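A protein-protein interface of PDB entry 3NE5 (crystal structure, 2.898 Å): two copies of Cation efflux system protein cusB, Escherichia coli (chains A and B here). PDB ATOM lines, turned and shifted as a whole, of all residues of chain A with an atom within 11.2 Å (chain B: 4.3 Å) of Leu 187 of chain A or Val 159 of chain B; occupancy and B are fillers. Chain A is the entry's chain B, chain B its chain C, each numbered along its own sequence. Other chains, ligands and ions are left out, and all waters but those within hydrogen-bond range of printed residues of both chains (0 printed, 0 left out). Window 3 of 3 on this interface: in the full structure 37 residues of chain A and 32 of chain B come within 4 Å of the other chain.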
ATOM      1  N   ALA A 126      22.281   6.268 -12.038  1.00  0.00           N
ATOM      2  CA  ALA A 126      21.976   5.087 -12.839  1.00  0.00           C
ATOM      3  C   ALA A 126      20.853   5.417 -13.814  1.00  0.00           C
ATOM      4  O   ALA A 126      20.063   6.327 -13.571  1.00  0.00           O
ATOM      5  CB  ALA A 126      21.581   3.926 -11.947  1.00  0.00           C
ATOM      6  N   ARG A 127      20.786   4.682 -14.917  1.00  0.00           N
ATOM      7  CA  ARG A 127      19.748   4.913 -15.917  1.00  0.00           C
ATOM      8  C   ARG A 127      18.514   4.069 -15.623  1.00  0.00           C
ATOM      9  O   ARG A 127      17.427   4.333 -16.140  1.00  0.00           O
ATOM     10  CB  ARG A 127      20.271   4.600 -17.315  1.00  0.00           C
ATOM     11  CG  ARG A 127      21.287   5.596 -17.839  1.00  0.00           C
ATOM     12  CD  ARG A 127      20.610   6.786 -18.495  1.00  0.00           C
ATOM     13  NE  ARG A 127      21.326   7.207 -19.696  1.00  0.00           N
ATOM     14  CZ  ARG A 127      22.096   8.287 -19.773  1.00  0.00           C
ATOM     15  NH1 ARG A 127      22.708   8.582 -20.913  1.00  0.00           N
ATOM     16  NH2 ARG A 127      22.250   9.075 -18.717  1.00  0.00           N
ATOM     17  N   ALA A 128      18.692   3.054 -14.788  1.00  0.00           N
ATOM     18  CA  ALA A 128      17.595   2.181 -14.402  1.00  0.00           C
ATOM     19  C   ALA A 128      17.892   1.555 -13.049  1.00  0.00           C
ATOM     20  O   ALA A 128      19.047   1.483 -12.633  1.00  0.00           O
ATOM     21  CB  ALA A 128      17.375   1.103 -15.453  1.00  0.00           C
ATOM     22  N   ASP A 157      16.682  -4.130 -16.477  1.00  0.00           N
ATOM     23  CA  ASP A 157      15.681  -3.437 -17.278  1.00  0.00           C
ATOM     24  C   ASP A 157      15.794  -3.736 -18.774  1.00  0.00           C
ATOM     25  O   ASP A 157      14.784  -3.872 -19.462  1.00  0.00           O
ATOM     26  CB  ASP A 157      15.748  -1.928 -17.039  1.00  0.00           C
ATOM     27  CG  ASP A 157      14.475  -1.217 -17.455  1.00  0.00           C
ATOM     28  OD1 ASP A 157      13.401  -1.570 -16.924  1.00  0.00           O
ATOM     29  OD2 ASP A 157      14.547  -0.303 -18.303  1.00  0.00           O
ATOM     30  N   TRP A 158      17.019  -3.848 -19.273  1.00  0.00           N
ATOM     31  CA  TRP A 158      17.233  -3.939 -20.716  1.00  0.00           C
ATOM     32  C   TRP A 158      17.427  -5.355 -21.258  1.00  0.00           C
ATOM     33  O   TRP A 158      17.585  -5.535 -22.462  1.00  0.00           O
ATOM     34  CB  TRP A 158      18.425  -3.077 -21.136  1.00  0.00           C
ATOM     35  CG  TRP A 158      18.415  -1.686 -20.582  1.00  0.00           C
ATOM     36  CD1 TRP A 158      17.444  -0.743 -20.748  1.00  0.00           C
ATOM     37  CD2 TRP A 158      19.440  -1.071 -19.792  1.00  0.00           C
ATOM     38  NE1 TRP A 158      17.795   0.416 -20.100  1.00  0.00           N
ATOM     39  CE2 TRP A 158      19.017   0.239 -19.506  1.00  0.00           C
ATOM     40  CE3 TRP A 158      20.671  -1.506 -19.296  1.00  0.00           C
ATOM     41  CZ2 TRP A 158      19.782   1.119 -18.746  1.00  0.00           C
ATOM     42  CZ3 TRP A 158      21.427  -0.633 -18.542  1.00  0.00           C
ATOM     43  CH2 TRP A 158      20.981   0.664 -18.274  1.00  0.00           C
ATOM     44  N   ALA A 161      14.827  -6.760 -23.925  1.00  0.00           N
ATOM     45  CA  ALA A 161      15.002  -6.166 -25.245  1.00  0.00           C
ATOM     46  C   ALA A 161      16.311  -6.606 -25.893  1.00  0.00           C
ATOM     47  O   ALA A 161      16.405  -6.684 -27.117  1.00  0.00           O
ATOM     48  CB  ALA A 161      14.935  -4.653 -25.159  1.00  0.00           C
ATOM     49  N   THR A 178      16.533  -4.208 -36.749  1.00  0.00           N
ATOM     50  CA  THR A 178      17.642  -4.245 -35.806  1.00  0.00           C
ATOM     51  C   THR A 178      17.975  -2.839 -35.311  1.00  0.00           C
ATOM     52  O   THR A 178      18.113  -2.612 -34.109  1.00  0.00           O
ATOM     53  CB  THR A 178      18.889  -4.879 -36.446  1.00  0.00           C
ATOM     54  OG1 THR A 178      18.496  -5.993 -37.255  1.00  0.00           O
ATOM     55  CG2 THR A 178      19.854  -5.354 -35.373  1.00  0.00           C
ATOM     56  N   GLU A 179      18.102  -1.898 -36.241  1.00  0.00           N
ATOM     57  CA  GLU A 179      18.303  -0.501 -35.879  1.00  0.00           C
ATOM     58  C   GLU A 179      17.195  -0.058 -34.929  1.00  0.00           C
ATOM     59  O   GLU A 179      17.406   0.786 -34.060  1.00  0.00           O
ATOM     60  CB  GLU A 179      18.309   0.385 -37.125  1.00  0.00           C
ATOM     61  CG  GLU A 179      19.486   0.148 -38.058  1.00  0.00           C
ATOM     62  CD  GLU A 179      19.319   0.847 -39.395  1.00  0.00           C
ATOM     63  OE1 GLU A 179      18.168   0.972 -39.863  1.00  0.00           O
ATOM     64  OE2 GLU A 179      20.341   1.266 -39.979  1.00  0.00           O
ATOM     65  N   GLY A 180      16.015  -0.645 -35.103  1.00  0.00           N
ATOM     66  CA  GLY A 180      14.864  -0.322 -34.280  1.00  0.00           C
ATOM     67  C   GLY A 180      15.007  -0.791 -32.846  1.00  0.00           C
ATOM     68  O   GLY A 180      14.866  -0.003 -31.912  1.00  0.00           O
ATOM     69  N   ILE A 181      15.282  -2.079 -32.665  1.00  0.00           N
ATOM     70  CA  ILE A 181      15.480  -2.626 -31.329  1.00  0.00           C
ATOM     71  C   ILE A 181      16.667  -1.946 -30.650  1.00  0.00           C
ATOM     72  O   ILE A 181      16.669  -1.748 -29.435  1.00  0.00           O
ATOM     73  CB  ILE A 181      15.690  -4.157 -31.360  1.00  0.00           C
ATOM     74  CG1 ILE A 181      15.733  -4.722 -29.940  1.00  0.00           C
ATOM     75  CG2 ILE A 181      16.960  -4.511 -32.111  1.00  0.00           C
ATOM     76  CD1 ILE A 181      14.465  -4.486 -29.152  1.00  0.00           C
ATOM     77  N   LEU A 182      17.669  -1.581 -31.442  1.00  0.00           N
ATOM     78  CA  LEU A 182      18.831  -0.867 -30.925  1.00  0.00           C
ATOM     79  C   LEU A 182      18.466   0.544 -30.476  1.00  0.00           C
ATOM     80  O   LEU A 182      19.005   1.046 -29.492  1.00  0.00           O
ATOM     81  CB  LEU A 182      19.945  -0.821 -31.973  1.00  0.00           C
ATOM     82  CG  LEU A 182      21.106  -1.800 -31.780  1.00  0.00           C
ATOM     83  CD1 LEU A 182      20.707  -2.974 -30.897  1.00  0.00           C
ATOM     84  CD2 LEU A 182      21.630  -2.274 -33.128  1.00  0.00           C
ATOM     85  N   GLU A 183      17.554   1.178 -31.203  1.00  0.00           N
ATOM     86  CA  GLU A 183      17.100   2.519 -30.849  1.00  0.00           C
ATOM     87  C   GLU A 183      16.212   2.518 -29.612  1.00  0.00           C
ATOM     88  O   GLU A 183      16.209   3.478 -28.845  1.00  0.00           O
ATOM     89  CB  GLU A 183      16.372   3.179 -32.022  1.00  0.00           C
ATOM     90  CG  GLU A 183      17.153   4.306 -32.668  1.00  0.00           C
ATOM     91  CD  GLU A 183      17.087   5.589 -31.860  1.00  0.00           C
ATOM     92  OE1 GLU A 183      16.034   5.843 -31.238  1.00  0.00           O
ATOM     93  OE2 GLU A 183      18.081   6.342 -31.850  1.00  0.00           O
ATOM     94  N   ARG A 184      15.457   1.441 -29.420  1.00  0.00           N
ATOM     95  CA  ARG A 184      14.607   1.327 -28.243  1.00  0.00           C
ATOM     96  C   ARG A 184      15.459   1.080 -27.002  1.00  0.00           C
ATOM     97  O   ARG A 184      15.052   1.393 -25.884  1.00  0.00           O
ATOM     98  CB  ARG A 184      13.561   0.221 -28.422  1.00  0.00           C
ATOM     99  CG  ARG A 184      12.652   0.427 -29.627  1.00  0.00           C
ATOM    100  CD  ARG A 184      11.300  -0.256 -29.458  1.00  0.00           C
ATOM    101  NE  ARG A 184      11.381  -1.713 -29.523  1.00  0.00           N
ATOM    102  CZ  ARG A 184      11.348  -2.512 -28.460  1.00  0.00           C
ATOM    103  NH1 ARG A 184      11.237  -1.997 -27.242  1.00  0.00           N
ATOM    104  NH2 ARG A 184      11.423  -3.827 -28.614  1.00  0.00           N
ATOM    105  N   LEU A 185      16.646   0.521 -27.209  1.00  0.00           N
ATOM    106  CA  LEU A 185      17.592   0.308 -26.120  1.00  0.00           C
ATOM    107  C   LEU A 185      18.174   1.623 -25.623  1.00  0.00           C
ATOM    108  O   LEU A 185      18.159   1.901 -24.426  1.00  0.00           O
ATOM    109  CB  LEU A 185      18.718  -0.630 -26.558  1.00  0.00           C
ATOM    110  CG  LEU A 185      18.747  -2.024 -25.927  1.00  0.00           C
ATOM    111  CD1 LEU A 185      17.391  -2.405 -25.365  1.00  0.00           C
ATOM    112  CD2 LEU A 185      19.243  -3.058 -26.928  1.00  0.00           C
ATOM    113  N   ARG A 186      18.690   2.431 -26.543  1.00  0.00           N
ATOM    114  CA  ARG A 186      19.319   3.686 -26.155  1.00  0.00           C
ATOM    115  C   ARG A 186      18.281   4.671 -25.625  1.00  0.00           C
ATOM    116  O   ARG A 186      18.589   5.507 -24.777  1.00  0.00           O
ATOM    117  CB  ARG A 186      20.111   4.295 -27.315  1.00  0.00           C
ATOM    118  CG  ARG A 186      19.304   5.218 -28.201  1.00  0.00           C
ATOM    119  CD  ARG A 186      20.192   6.241 -28.888  1.00  0.00           C
ATOM    120  NE  ARG A 186      19.391   7.234 -29.598  1.00  0.00           N
ATOM    121  CZ  ARG A 186      18.961   8.370 -29.061  1.00  0.00           C
ATOM    122  NH1 ARG A 186      19.262   8.670 -27.805  1.00  0.00           N
ATOM    123  NH2 ARG A 186      18.231   9.210 -29.782  1.00  0.00           N
ATOM    124  N   LEU A 187      17.051   4.567 -26.124  1.00  0.00           N
ATOM    125  CA  LEU A 187      15.946   5.362 -25.599  1.00  0.00           C
ATOM    126  C   LEU A 187      15.577   4.869 -24.205  1.00  0.00           C
ATOM    127  O   LEU A 187      15.096   5.634 -23.369  1.00  0.00           O
ATOM    128  CB  LEU A 187      14.728   5.290 -26.522  1.00  0.00           C
ATOM    129  CG  LEU A 187      14.792   6.074 -27.833  1.00  0.00           C
ATOM    130  CD1 LEU A 187      13.482   5.950 -28.599  1.00  0.00           C
ATOM    131  CD2 LEU A 187      15.122   7.532 -27.571  1.00  0.00           C
ATOM    132  N   ALA A 188      15.804   3.580 -23.966  1.00  0.00           N
ATOM    133  CA  ALA A 188      15.556   2.983 -22.661  1.00  0.00           C
ATOM    134  C   ALA A 188      16.624   3.417 -21.666  1.00  0.00           C
ATOM    135  O   ALA A 188      16.536   3.116 -20.474  1.00  0.00           O
ATOM    136  CB  ALA A 188      15.514   1.467 -22.767  1.00  0.00           C
ATOM    137  N   GLY A 189      17.638   4.117 -22.164  1.00  0.00           N
ATOM    138  CA  GLY A 189      18.666   4.677 -21.308  1.00  0.00           C
ATOM    139  C   GLY A 189      19.991   3.943 -21.335  1.00  0.00           C
ATOM    140  O   GLY A 189      20.998   4.464 -20.858  1.00  0.00           O
ATOM    141  N   MET A 190      19.996   2.733 -21.887  1.00  0.00           N
ATOM    142  CA  MET A 190      21.216   1.929 -21.945  1.00  0.00           C
ATOM    143  C   MET A 190      22.330   2.676 -22.677  1.00  0.00           C
ATOM    144  O   MET A 190      22.173   3.056 -23.835  1.00  0.00           O
ATOM    145  CB  MET A 190      20.945   0.577 -22.609  1.00  0.00           C
ATOM    146  CG  MET A 190      22.157  -0.337 -22.686  1.00  0.00           C
ATOM    147  SD  MET A 190      21.750  -1.968 -23.339  1.00  0.00           S
ATOM    148  CE  MET A 190      23.376  -2.713 -23.449  1.00  0.00           C
ATOM    149  N   PRO A 191      23.461   2.893 -21.990  1.00  0.00           N
ATOM    150  CA  PRO A 191      24.590   3.676 -22.506  1.00  0.00           C
ATOM    151  C   PRO A 191      25.093   3.170 -23.853  1.00  0.00           C
ATOM    152  O   PRO A 191      25.206   1.962 -24.057  1.00  0.00           O
ATOM    153  CB  PRO A 191      25.666   3.480 -21.436  1.00  0.00           C
ATOM    154  CG  PRO A 191      24.908   3.181 -20.192  1.00  0.00           C
ATOM    155  CD  PRO A 191      23.717   2.384 -20.633  1.00  0.00           C
ATOM    156  N   GLU A 192      25.401   4.096 -24.755  1.00  0.00           N
ATOM    157  CA  GLU A 192      25.865   3.754 -26.097  1.00  0.00           C
ATOM    158  C   GLU A 192      27.071   2.815 -26.087  1.00  0.00           C
ATOM    159  O   GLU A 192      27.199   1.952 -26.954  1.00  0.00           O
ATOM    160  CB  GLU A 192      26.174   5.024 -26.896  1.00  0.00           C
ATOM    161  CG  GLU A 192      24.972   5.945 -27.077  1.00  0.00           C
ATOM    162  CD  GLU A 192      25.201   7.021 -28.123  1.00  0.00           C
ATOM    163  OE1 GLU A 192      26.153   7.815 -27.971  1.00  0.00           O
ATOM    164  OE2 GLU A 192      24.419   7.078 -29.096  1.00  0.00           O
ATOM    165  N   ALA A 193      27.950   2.983 -25.105  1.00  0.00           N
ATOM    166  CA  ALA A 193      29.132   2.133 -24.989  1.00  0.00           C
ATOM    167  C   ALA A 193      28.747   0.702 -24.633  1.00  0.00           C
ATOM    168  O   ALA A 193      29.368  -0.253 -25.098  1.00  0.00           O
ATOM    169  CB  ALA A 193      30.094   2.695 -23.957  1.00  0.00           C
ATOM    170  N   ILE A 195      25.798  -0.674 -25.346  1.00  0.00           N
ATOM    171  CA  ILE A 195      25.116  -1.220 -26.512  1.00  0.00           C
ATOM    172  C   ILE A 195      26.131  -1.862 -27.453  1.00  0.00           C
ATOM    173  O   ILE A 195      25.871  -2.915 -28.039  1.00  0.00           O
ATOM    174  CB  ILE A 195      24.330  -0.135 -27.276  1.00  0.00           C
ATOM    175  CG1 ILE A 195      23.250   0.475 -26.380  1.00  0.00           C
ATOM    176  CG2 ILE A 195      23.705  -0.712 -28.536  1.00  0.00           C
ATOM    177  CD1 ILE A 195      22.409   1.532 -27.072  1.00  0.00           C
ATOM    178  N   LYS A 231      17.076   5.416  -9.547  1.00  0.00           N
ATOM    179  CA  LYS A 231      17.458   6.371 -10.580  1.00  0.00           C
ATOM    180  C   LYS A 231      17.625   7.784 -10.031  1.00  0.00           C
ATOM    181  O   LYS A 231      18.212   8.644 -10.688  1.00  0.00           O
ATOM    182  CB  LYS A 231      16.438   6.377 -11.717  1.00  0.00           C
ATOM    183  CG  LYS A 231      15.785   5.036 -11.973  1.00  0.00           C
ATOM    184  CD  LYS A 231      15.395   4.906 -13.433  1.00  0.00           C
ATOM    185  CE  LYS A 231      14.941   6.238 -14.002  1.00  0.00           C
ATOM    186  NZ  LYS A 231      14.476   6.097 -15.408  1.00  0.00           N
ATOM    187  N   PHE B 131      16.602  11.588 -19.789  1.00  0.00           N
ATOM    188  CA  PHE B 131      17.932  11.758 -19.218  1.00  0.00           C
ATOM    189  C   PHE B 131      18.694  12.908 -19.861  1.00  0.00           C
ATOM    190  O   PHE B 131      18.505  13.216 -21.037  1.00  0.00           O
ATOM    191  CB  PHE B 131      18.738  10.456 -19.295  1.00  0.00           C
ATOM    192  CG  PHE B 131      18.750   9.826 -20.658  1.00  0.00           C
ATOM    193  CD1 PHE B 131      19.691  10.203 -21.601  1.00  0.00           C
ATOM    194  CD2 PHE B 131      17.824   8.852 -20.995  1.00  0.00           C
ATOM    195  CE1 PHE B 131      19.705   9.624 -22.856  1.00  0.00           C
ATOM    196  CE2 PHE B 131      17.836   8.270 -22.248  1.00  0.00           C
ATOM    197  CZ  PHE B 131      18.777   8.657 -23.179  1.00  0.00           C
ATOM    198  N   THR B 154      16.933  13.755 -23.549  1.00  0.00           N
ATOM    199  CA  THR B 154      16.289  12.777 -24.417  1.00  0.00           C
ATOM    200  C   THR B 154      14.986  12.294 -23.794  1.00  0.00           C
ATOM    201  O   THR B 154      14.968  11.832 -22.655  1.00  0.00           O
ATOM    202  CB  THR B 154      17.199  11.563 -24.669  1.00  0.00           C
ATOM    203  OG1 THR B 154      18.257  11.929 -25.564  1.00  0.00           O
ATOM    204  CG2 THR B 154      16.405  10.419 -25.278  1.00  0.00           C
ATOM    205  N   ILE B 155      13.896  12.403 -24.545  1.00  0.00           N
ATOM    206  CA  ILE B 155      12.581  12.024 -24.044  1.00  0.00           C
ATOM    207  C   ILE B 155      11.918  10.995 -24.945  1.00  0.00           C
ATOM    208  O   ILE B 155      11.515  11.310 -26.064  1.00  0.00           O
ATOM    209  CB  ILE B 155      11.657  13.243 -23.934  1.00  0.00           C
ATOM    210  CG1 ILE B 155      12.278  14.301 -23.023  1.00  0.00           C
ATOM    211  CG2 ILE B 155      10.293  12.829 -23.413  1.00  0.00           C
ATOM    212  CD1 ILE B 155      11.405  15.518 -22.841  1.00  0.00           C
ATOM    213  N   PRO B 156      11.810   9.752 -24.457  1.00  0.00           N
ATOM    214  CA  PRO B 156      11.250   8.629 -25.216  1.00  0.00           C
ATOM    215  C   PRO B 156       9.726   8.545 -25.150  1.00  0.00           C
ATOM    216  O   PRO B 156       9.146   7.637 -25.740  1.00  0.00           O
ATOM    217  CB  PRO B 156      11.859   7.414 -24.512  1.00  0.00           C
ATOM    218  CG  PRO B 156      12.042   7.880 -23.111  1.00  0.00           C
ATOM    219  CD  PRO B 156      12.528   9.288 -23.257  1.00  0.00           C
ATOM    220  N   ASP B 157       9.090   9.475 -24.447  1.00  0.00           N
ATOM    221  CA  ASP B 157       7.651   9.398 -24.222  1.00  0.00           C
ATOM    222  C   ASP B 157       6.829   9.590 -25.495  1.00  0.00           C
ATOM    223  O   ASP B 157       5.763   8.997 -25.648  1.00  0.00           O
ATOM    224  CB  ASP B 157       7.219  10.418 -23.168  1.00  0.00           C
ATOM    225  CG  ASP B 157       5.808  10.175 -22.671  1.00  0.00           C
ATOM    226  OD1 ASP B 157       5.491   9.012 -22.341  1.00  0.00           O
ATOM    227  OD2 ASP B 157       5.018  11.142 -22.607  1.00  0.00           O
ATOM    228  N   TRP B 158       7.331  10.413 -26.410  1.00  0.00           N
ATOM    229  CA  TRP B 158       6.553  10.798 -27.582  1.00  0.00           C
ATOM    230  C   TRP B 158       6.948  10.094 -28.879  1.00  0.00           C
ATOM    231  O   TRP B 158       6.431  10.435 -29.940  1.00  0.00           O
ATOM    232  CB  TRP B 158       6.633  12.312 -27.800  1.00  0.00           C
ATOM    233  CG  TRP B 158       6.337  13.134 -26.581  1.00  0.00           C
ATOM    234  CD1 TRP B 158       5.226  13.061 -25.793  1.00  0.00           C
ATOM    235  CD2 TRP B 158       7.153  14.173 -26.026  1.00  0.00           C
ATOM    236  NE1 TRP B 158       5.305  13.978 -24.774  1.00  0.00           N
ATOM    237  CE2 TRP B 158       6.479  14.674 -24.896  1.00  0.00           C
ATOM    238  CE3 TRP B 158       8.391  14.722 -26.371  1.00  0.00           C
ATOM    239  CZ2 TRP B 158       7.002  15.698 -24.109  1.00  0.00           C
ATOM    240  CZ3 TRP B 158       8.907  15.737 -25.589  1.00  0.00           C
ATOM    241  CH2 TRP B 158       8.214  16.214 -24.473  1.00  0.00           C
ATOM    242  N   VAL B 159       7.854   9.123 -28.816  1.00  0.00           N
ATOM    243  CA  VAL B 159       8.353   8.510 -30.049  1.00  0.00           C
ATOM    244  C   VAL B 159       7.341   7.583 -30.725  1.00  0.00           C
ATOM    245  O   VAL B 159       7.292   7.506 -31.952  1.00  0.00           O
ATOM    246  CB  VAL B 159       9.695   7.758 -29.853  1.00  0.00           C
ATOM    247  CG1 VAL B 159      10.624   8.553 -28.949  1.00  0.00           C
ATOM    248  CG2 VAL B 159       9.458   6.362 -29.303  1.00  0.00           C
ATOM    249  N   GLU B 160       6.537   6.884 -29.929  1.00  0.00           N
ATOM    250  CA  GLU B 160       5.551   5.955 -30.476  1.00  0.00           C
ATOM    251  C   GLU B 160       4.509   6.690 -31.311  1.00  0.00           C
ATOM    252  O   GLU B 160       4.258   6.340 -32.464  1.00  0.00           O
ATOM    253  CB  GLU B 160       4.868   5.160 -29.357  1.00  0.00           C
ATOM    254  CG  GLU B 160       5.790   4.218 -28.595  1.00  0.00           C
ATOM    255  CD  GLU B 160       6.650   4.936 -27.567  1.00  0.00           C
ATOM    256  OE1 GLU B 160       7.799   4.498 -27.339  1.00  0.00           O
ATOM    257  OE2 GLU B 160       6.177   5.937 -26.986  1.00  0.00           O
ATOM    258  N   ALA B 161       3.908   7.715 -30.716  1.00  0.00           N
ATOM    259  CA  ALA B 161       2.892   8.508 -31.396  1.00  0.00           C
ATOM    260  C   ALA B 161       3.481   9.295 -32.560  1.00  0.00           C
ATOM    261  O   ALA B 161       2.823   9.491 -33.580  1.00  0.00           O
ATOM    262  CB  ALA B 161       2.208   9.439 -30.414  1.00  0.00           C
ATOM    263  N   GLN B 162       4.720   9.749 -32.406  1.00  0.00           N
ATOM    264  CA  GLN B 162       5.400  10.459 -33.483  1.00  0.00           C
ATOM    265  C   GLN B 162       5.531   9.575 -34.715  1.00  0.00           C
ATOM    266  O   GLN B 162       5.173   9.983 -35.817  1.00  0.00           O
ATOM    267  CB  GLN B 162       6.784  10.934 -33.042  1.00  0.00           C
ATOM    268  CG  GLN B 162       6.784  12.219 -32.238  1.00  0.00           C
ATOM    269  CD  GLN B 162       8.176  12.785 -32.063  1.00  0.00           C
ATOM    270  OE1 GLN B 162       8.736  13.378 -32.983  1.00  0.00           O
ATOM    271  NE2 GLN B 162       8.743  12.608 -30.877  1.00  0.00           N
ATOM    272  N   SER B 163       6.048   8.366 -34.521  1.00  0.00           N
ATOM    273  CA  SER B 163       6.230   7.429 -35.623  1.00  0.00           C
ATOM    274  C   SER B 163       4.886   7.022 -36.214  1.00  0.00           C
ATOM    275  O   SER B 163       4.772   6.781 -37.416  1.00  0.00           O
ATOM    276  CB  SER B 163       7.000   6.189 -35.163  1.00  0.00           C
ATOM    277  OG  SER B 163       6.245   5.436 -34.231  1.00  0.00           O
ATOM    278  N   ILE B 204      11.462  11.629 -36.469  1.00  0.00           N
ATOM    279  CA  ILE B 204      11.117  11.420 -35.069  1.00  0.00           C
ATOM    280  C   ILE B 204      12.032  12.224 -34.153  1.00  0.00           C
ATOM    281  O   ILE B 204      13.257  12.162 -34.268  1.00  0.00           O
ATOM    282  CB  ILE B 204      11.195   9.931 -34.682  1.00  0.00           C
ATOM    283  CG1 ILE B 204      10.126   9.127 -35.419  1.00  0.00           C
ATOM    284  CG2 ILE B 204      11.022   9.762 -33.183  1.00  0.00           C
ATOM    285  CD1 ILE B 204       9.998   7.704 -34.924  1.00  0.00           C
ATOM    286  N   THR B 206      13.710  12.949 -30.649  1.00  0.00           N
ATOM    287  CA  THR B 206      14.105  12.245 -29.435  1.00  0.00           C
ATOM    288  C   THR B 206      14.917  13.142 -28.498  1.00  0.00           C
ATOM    289  O   THR B 206      14.734  13.109 -27.283  1.00  0.00           O
ATOM    290  CB  THR B 206      14.891  10.959 -29.764  1.00  0.00           C
ATOM    291  OG1 THR B 206      15.897  10.741 -28.769  1.00  0.00           O
ATOM    292  CG2 THR B 206      15.561  11.079 -31.125  1.00  0.00           C
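NH2 of Arg 186 of chain A is in hydrogen-bond range of OG1 of Thr 206 of chain B, 3.0 Å away.
O of Gly 189 of chain A sits at hydrogen-bond distance from NE of Arg 127 of chain A. The side-chain carboxylate (OE2) of Glu 183 of chain A lies within salt-bridge range of the guanidinium group (NE) of Arg 186 of chain A. O of Phe 131 of chain B lies within hydrogen-bond range of N of Thr 154 of chain B, 3.0 Å away. The backbone NH (N) of Ile 155 of chain B lies within hydrogen-bond range of the backbone carbonyl oxygen (O) of Thr 206 of chain B (2.9 Å). The side-chain hydroxyl (OG) of Ser 163 of chain B sits at hydrogen-bond distance from the backbone carbonyl oxygen (O) of Val 159 of chain B, at 3.3 Å.
Among the printed residues, merely in contact across the chains: Arg 127 of chain A with Phe 131 of chain B, Leu 187 of chain A with Thr 206 of chain B, Arg 186 of chain A with Phe 131 of chain B, Leu 187 of chain A with Pro 156 of chain B, Gly 189 of chain A with Phe 131 of chain B, Leu 187 of chain A with Val 159 of chain B, Leu 187 of chain A with Thr 154 of chain B and Leu 187 of chain A with Phe 131 of chain B.
Of the printed residues of chain A, Val 159 of chain B touches Leu 187 (3.9 Å). Printed residues of chain A within 4 Å of Pro 156 of chain B: Leu 187 (3.8 Å). No residue of chain A comes within 4 Å of Asp 157 of chain B. No residue of chain A comes within 4 Å of Ala 161 of chain B. No residue of chain A comes within 4 Å of Gln 162 of chain B. No residue of chain A comes within 4 Å of Ser 163 of chain B. Thr 206 of chain B touches just these residues of chain A: Arg 186 (3.0 Å) and Leu 187 (3.5 Å). Printed residues of chain B within 4 Å of Arg 186 of chain A: Phe 131 (3.5 Å) and Thr 206 (3.0 Å). Printed residues of chain A within 4 Å of Phe 131 of chain B: Arg 127, Arg 186, Leu 187 and Gly 189. Of the printed residues of chain A, Thr 154 of chain B touches Leu 187. Ile 155 of chain B touches none of the printed residues of chain A. Gly 180 of chain A touches none of the printed residues of chain B. The nearest printed residue of chain B that does not touch Leu 187 of chain A is Ile 155 of chain B (5.4 Å). The nearest residue of chain A that does not touch Val 159 of chain B is Glu 183 of chain A (6.5 Å). The nearest printed residue of chain A that does not touch Phe 131 of chain B is Ala 188 of chain A (5.0 Å).
Of the 24 printed residues of chain A, 4 touch a printed residue of chain B. Hydrophobic or aromatic side chains of chain A within 4 Å of the printed part of chain B: Leu 187. Hydrophobic or aromatic side chains of chain B within 4 Å of the printed part of chain A: Phe 131, Pro 156 and Val 159. Among the printed residues, 9 pairs touch across the chains. Among the printed residues, no Asp or Glu carboxylate lies within 4 Å of a Lys or Arg side-chain nitrogen of the other chain.
3 positions are printed for both chains.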
